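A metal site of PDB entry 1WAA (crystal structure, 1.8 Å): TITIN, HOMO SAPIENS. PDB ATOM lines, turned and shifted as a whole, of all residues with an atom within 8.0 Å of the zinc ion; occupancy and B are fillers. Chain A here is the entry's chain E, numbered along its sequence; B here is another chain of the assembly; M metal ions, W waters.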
ATOM      1  N   THR A  22      -6.213  23.308  -9.832  1.00  0.00           N
ATOM      2  CA  THR A  22      -5.879  22.629  -8.601  1.00  0.00           C
ATOM      3  C   THR A  22      -6.033  23.537  -7.396  1.00  0.00           C
ATOM      4  O   THR A  22      -5.819  24.755  -7.486  1.00  0.00           O
ATOM      5  CB  THR A  22      -4.495  21.914  -8.654  1.00  0.00           C
ATOM      6  OG1 THR A  22      -3.578  22.488  -7.711  1.00  0.00           O
ATOM      7  CG2 THR A  22      -3.900  21.958 -10.036  1.00  0.00           C
ATOM      8  N   HIS A  24      -5.055  23.918  -3.230  1.00  0.00           N
ATOM      9  CA  HIS A  24      -4.076  23.512  -2.220  1.00  0.00           C
ATOM     10  C   HIS A  24      -4.640  23.962  -0.903  1.00  0.00           C
ATOM     11  O   HIS A  24      -5.105  25.090  -0.796  1.00  0.00           O
ATOM     12  CB  HIS A  24      -2.750  24.235  -2.440  1.00  0.00           C
ATOM     13  CG  HIS A  24      -2.194  24.078  -3.835  1.00  0.00           C
ATOM     14  ND1 HIS A  24      -2.327  25.052  -4.795  1.00  0.00           N
ATOM     15  CD2 HIS A  24      -1.505  23.062  -4.409  1.00  0.00           C
ATOM     16  CE1 HIS A  24      -1.752  24.636  -5.925  1.00  0.00           C
ATOM     17  NE2 HIS A  24      -1.253  23.436  -5.716  1.00  0.00           N
ATOM     18  N   SER A  48      -3.218   9.898  -4.244  1.00  0.00           N
ATOM     19  CA  SER A  48      -3.187   9.558  -5.676  1.00  0.00           C
ATOM     20  C   SER A  48      -2.381  10.600  -6.456  1.00  0.00           C
ATOM     21  O   SER A  48      -1.893  11.581  -5.869  1.00  0.00           O
ATOM     22  CB  SER A  48      -4.603   9.522  -6.258  1.00  0.00           C
ATOM     23  OG  SER A  48      -5.394   8.545  -5.584  1.00  0.00           O
ATOM     24  N   PRO A  49      -2.242  10.396  -7.780  1.00  0.00           N
ATOM     25  CA  PRO A  49      -1.649  11.456  -8.609  1.00  0.00           C
ATOM     26  C   PRO A  49      -2.422  12.770  -8.512  1.00  0.00           C
ATOM     27  O   PRO A  49      -1.812  13.831  -8.427  1.00  0.00           O
ATOM     28  CB  PRO A  49      -1.728  10.889 -10.025  1.00  0.00           C
ATOM     29  CG  PRO A  49      -1.774   9.414  -9.806  1.00  0.00           C
ATOM     30  CD  PRO A  49      -2.578   9.209  -8.572  1.00  0.00           C
ATOM     31  N   ASP A  50      -3.751  12.680  -8.509  1.00  0.00           N
ATOM     32  CA  ASP A  50      -4.625  13.866  -8.449  1.00  0.00           C
ATOM     33  C   ASP A  50      -4.969  14.306  -7.014  1.00  0.00           C
ATOM     34  O   ASP A  50      -5.623  15.320  -6.812  1.00  0.00           O
ATOM     35  CB  ASP A  50      -5.914  13.616  -9.263  1.00  0.00           C
ATOM     36  CG  ASP A  50      -5.629  13.301 -10.754  1.00  0.00           C
ATOM     37  OD1 ASP A  50      -4.558  13.715 -11.276  1.00  0.00           O
ATOM     38  OD2 ASP A  50      -6.455  12.632 -11.446  1.00  0.00           O
ATOM     39  N   CYS A  51      -4.512  13.541  -6.020  1.00  0.00           N
ATOM     40  CA  CYS A  51      -4.870  13.803  -4.640  1.00  0.00           C
ATOM     41  C   CYS A  51      -3.668  13.555  -3.738  1.00  0.00           C
ATOM     42  O   CYS A  51      -3.453  12.444  -3.260  1.00  0.00           O
ATOM     43  CB  CYS A  51      -6.041  12.928  -4.235  1.00  0.00           C
ATOM     44  SG  CYS A  51      -6.495  13.181  -2.531  1.00  0.00           S
ATOM     45  N   GLU A  52      -2.867  14.600  -3.539  1.00  0.00           N
ATOM     46  CA  GLU A  52      -1.540  14.431  -2.911  1.00  0.00           C
ATOM     47  C   GLU A  52      -1.605  14.918  -1.467  1.00  0.00           C
ATOM     48  O   GLU A  52      -2.082  16.010  -1.187  1.00  0.00           O
ATOM     49  CB  GLU A  52      -0.473  15.184  -3.706  1.00  0.00           C
ATOM     50  CG  GLU A  52      -0.138  14.501  -5.037  1.00  0.00           C
ATOM     51  CD  GLU A  52       0.485  15.411  -6.094  1.00  0.00           C
ATOM     52  OE1 GLU A  52       0.272  16.636  -6.063  1.00  0.00           O
ATOM     53  OE2 GLU A  52       1.157  14.903  -7.008  1.00  0.00           O
ATOM     54  N   ILE A  54       0.590  15.682   1.854  1.00  0.00           N
ATOM     55  CA  ILE A  54       1.959  16.145   2.123  1.00  0.00           C
ATOM     56  C   ILE A  54       2.098  16.482   3.596  1.00  0.00           C
ATOM     57  O   ILE A  54       1.179  17.090   4.198  1.00  0.00           O
ATOM     58  CB  ILE A  54       2.242  17.450   1.284  1.00  0.00           C
ATOM     59  CG1 ILE A  54       2.015  17.229  -0.236  1.00  0.00           C
ATOM     60  CG2 ILE A  54       3.617  18.102   1.647  1.00  0.00           C
ATOM     61  CD1 ILE A  54       3.028  16.397  -0.929  1.00  0.00           C
ATOM     62  N   ILE A  63      -3.098  18.642  -1.781  1.00  0.00           N
ATOM     63  CA  ILE A  63      -3.221  19.132  -3.161  1.00  0.00           C
ATOM     64  C   ILE A  63      -4.243  18.296  -3.957  1.00  0.00           C
ATOM     65  O   ILE A  63      -4.142  17.076  -3.999  1.00  0.00           O
ATOM     66  CB  ILE A  63      -1.875  19.145  -3.940  1.00  0.00           C
ATOM     67  CG1 ILE A  63      -0.747  19.716  -3.076  1.00  0.00           C
ATOM     68  CG2 ILE A  63      -2.037  19.985  -5.226  1.00  0.00           C
ATOM     69  CD1 ILE A  63       0.644  19.591  -3.701  1.00  0.00           C
ATOM     70  N   LEU A  64      -5.216  18.972  -4.550  1.00  0.00           N
ATOM     71  CA  LEU A  64      -6.232  18.323  -5.370  1.00  0.00           C
ATOM     72  C   LEU A  64      -6.183  18.941  -6.762  1.00  0.00           C
ATOM     73  O   LEU A  64      -6.453  20.120  -6.949  1.00  0.00           O
ATOM     74  CB  LEU A  64      -7.623  18.489  -4.733  1.00  0.00           C
ATOM     75  CG  LEU A  64      -7.835  18.131  -3.256  1.00  0.00           C
ATOM     76  CD1 LEU A  64      -9.180  18.674  -2.744  1.00  0.00           C
ATOM     77  CD2 LEU A  64      -7.736  16.624  -2.998  1.00  0.00           C
ATOM     78  N   HIS A  65      -5.789  18.122  -7.732  1.00  0.00           N
ATOM     79  CA  HIS A  65      -5.615  18.520  -9.100  1.00  0.00           C
ATOM     80  C   HIS A  65      -6.886  18.281  -9.843  1.00  0.00           C
ATOM     81  O   HIS A  65      -7.680  17.409  -9.459  1.00  0.00           O
ATOM     82  CB  HIS A  65      -4.528  17.677  -9.729  1.00  0.00           C
ATOM     83  CG  HIS A  65      -3.156  18.022  -9.270  1.00  0.00           C
ATOM     84  ND1 HIS A  65      -2.499  19.164  -9.674  1.00  0.00           N
ATOM     85  CD2 HIS A  65      -2.285  17.361  -8.465  1.00  0.00           C
ATOM     86  CE1 HIS A  65      -1.297  19.206  -9.123  1.00  0.00           C
ATOM     87  NE2 HIS A  65      -1.149  18.111  -8.399  1.00  0.00           N
ATOM     88  N   LYS B  10       8.098  15.870 -12.679  1.00  0.00           N
ATOM     89  CA  LYS B  10       6.973  16.746 -12.943  1.00  0.00           C
ATOM     90  C   LYS B  10       7.486  18.144 -12.774  1.00  0.00           C
ATOM     91  O   LYS B  10       7.832  18.524 -11.648  1.00  0.00           O
ATOM     92  CB  LYS B  10       5.836  16.506 -11.956  1.00  0.00           C
ATOM     93  CG  LYS B  10       4.996  15.320 -12.300  1.00  0.00           C
ATOM     94  CD  LYS B  10       4.876  14.412 -11.095  1.00  0.00           C
ATOM     95  CE  LYS B  10       3.453  14.061 -10.774  1.00  0.00           C
ATOM     96  NZ  LYS B  10       2.994  12.885 -11.526  1.00  0.00           N
ATOM     97  N   TYR B  13       4.561  24.279 -12.921  1.00  0.00           N
ATOM     98  CA  TYR B  13       3.529  24.816 -13.786  1.00  0.00           C
ATOM     99  C   TYR B  13       3.418  26.301 -13.411  1.00  0.00           C
ATOM    100  O   TYR B  13       3.702  26.661 -12.268  1.00  0.00           O
ATOM    101  CB  TYR B  13       2.217  24.087 -13.521  1.00  0.00           C
ATOM    102  CG  TYR B  13       2.058  22.793 -14.305  1.00  0.00           C
ATOM    103  CD1 TYR B  13       1.075  22.660 -15.288  1.00  0.00           C
ATOM    104  CD2 TYR B  13       2.903  21.707 -14.085  1.00  0.00           C
ATOM    105  CE1 TYR B  13       0.913  21.469 -16.001  1.00  0.00           C
ATOM    106  CE2 TYR B  13       2.766  20.522 -14.830  1.00  0.00           C
ATOM    107  CZ  TYR B  13       1.763  20.416 -15.786  1.00  0.00           C
ATOM    108  OH  TYR B  13       1.640  19.244 -16.512  1.00  0.00           O
ATOM    109  N   GLU B  26       4.891  23.489  -7.181  1.00  0.00           N
ATOM    110  CA  GLU B  26       5.297  22.131  -6.848  1.00  0.00           C
ATOM    111  C   GLU B  26       6.100  21.518  -7.973  1.00  0.00           C
ATOM    112  O   GLU B  26       5.848  21.732  -9.168  1.00  0.00           O
ATOM    113  CB  GLU B  26       4.081  21.260  -6.543  1.00  0.00           C
ATOM    114  CG  GLU B  26       3.104  21.203  -7.652  1.00  0.00           C
ATOM    115  CD  GLU B  26       1.969  20.258  -7.424  1.00  0.00           C
ATOM    116  OE1 GLU B  26       2.223  19.040  -7.278  1.00  0.00           O
ATOM    117  OE2 GLU B  26       0.811  20.749  -7.388  1.00  0.00           O
ATOM    118  N   ILE B  27       7.070  20.730  -7.578  1.00  0.00           N
ATOM    119  CA  ILE B  27       7.886  20.013  -8.530  1.00  0.00           C
ATOM    120  C   ILE B  27       8.116  18.621  -7.918  1.00  0.00           C
ATOM    121  O   ILE B  27       8.139  18.485  -6.693  1.00  0.00           O
ATOM    122  CB  ILE B  27       9.211  20.819  -8.788  1.00  0.00           C
ATOM    123  CG1 ILE B  27      10.109  20.127  -9.826  1.00  0.00           C
ATOM    124  CG2 ILE B  27       9.987  21.046  -7.503  1.00  0.00           C
ATOM    125  CD1 ILE B  27      11.225  21.037 -10.375  1.00  0.00           C
ATOM    126  N   GLU B  28       8.268  17.621  -8.758  1.00  0.00           N
ATOM    127  CA  GLU B  28       8.571  16.306  -8.300  1.00  0.00           C
ATOM    128  C   GLU B  28       9.863  15.897  -8.968  1.00  0.00           C
ATOM    129  O   GLU B  28       9.983  16.018 -10.165  1.00  0.00           O
ATOM    130  CB  GLU B  28       7.464  15.317  -8.661  1.00  0.00           C
ATOM    131  CG  GLU B  28       7.543  13.911  -7.989  1.00  0.00           C
ATOM    132  CD  GLU B  28       6.334  13.062  -8.354  1.00  0.00           C
ATOM    133  OE1 GLU B  28       6.500  12.130  -9.182  1.00  0.00           O
ATOM    134  OE2 GLU B  28       5.203  13.372  -7.892  1.00  0.00           O
ATOM    135  N   LYS B  59       8.778  15.306  -3.564  1.00  0.00           N
ATOM    136  CA  LYS B  59       8.097  16.589  -3.780  1.00  0.00           C
ATOM    137  C   LYS B  59       8.755  17.781  -3.111  1.00  0.00           C
ATOM    138  O   LYS B  59       9.158  17.722  -1.960  1.00  0.00           O
ATOM    139  CB  LYS B  59       6.644  16.565  -3.326  1.00  0.00           C
ATOM    140  CG  LYS B  59       5.856  15.476  -3.903  1.00  0.00           C
ATOM    141  CD  LYS B  59       4.463  15.953  -4.289  1.00  0.00           C
ATOM    142  CE  LYS B  59       3.710  14.836  -5.031  1.00  0.00           C
ATOM    143  NZ  LYS B  59       3.860  14.923  -6.535  1.00  0.00           N
ATOM    144  N   ILE B  61       7.761  21.881  -2.465  1.00  0.00           N
ATOM    145  CA  ILE B  61       6.687  22.832  -2.579  1.00  0.00           C
ATOM    146  C   ILE B  61       7.120  24.213  -2.101  1.00  0.00           C
ATOM    147  O   ILE B  61       7.833  24.336  -1.108  1.00  0.00           O
ATOM    148  CB  ILE B  61       5.461  22.337  -1.780  1.00  0.00           C
ATOM    149  CG1 ILE B  61       4.812  21.162  -2.517  1.00  0.00           C
ATOM    150  CG2 ILE B  61       4.462  23.470  -1.535  1.00  0.00           C
ATOM    151  CD1 ILE B  61       4.213  20.156  -1.601  1.00  0.00           C
HETATM  152 ZN    ZN M   1       0.762  17.506  -7.735  1.00  0.00          ZN
HETATM  153  O   HOH W   1       1.829  16.542  -9.413  1.00  0.00           O
HETATM  154  O   HOH W   2       0.601  14.417  -9.356  1.00  0.00           O
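Water W2 bridges the side-chain carboxylate (OE2) of Glu 52 (2.5 Å) and the backbone carbonyl oxygen (O) of Pro 49 (2.7 Å).
Of the 18 residues printed, 3 come within 4 Å of the zinc ion.
NZ of Lys 59 of chain B is in salt-bridge range of OE2 of Glu 52, at 2.7 Å.
O of Ile 63 is in hydrogen-bond range of N of Glu 52 (2.8 Å).
N of His 65 sits at hydrogen-bond distance from O of Asp 50 (3.0 Å).
OE1 of Glu 52 binds the zinc ion (1.9 Å).
The zinc ion is bound by NE2 of His 65 (2.1 Å).
OE1 of Glu 26 of chain B binds the zinc ion (2.2 Å).
Water W1 binds the zinc ion (2.2 Å).
Slightly farther from the zinc ion lies OE2 of Glu 52 (2.7 Å).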
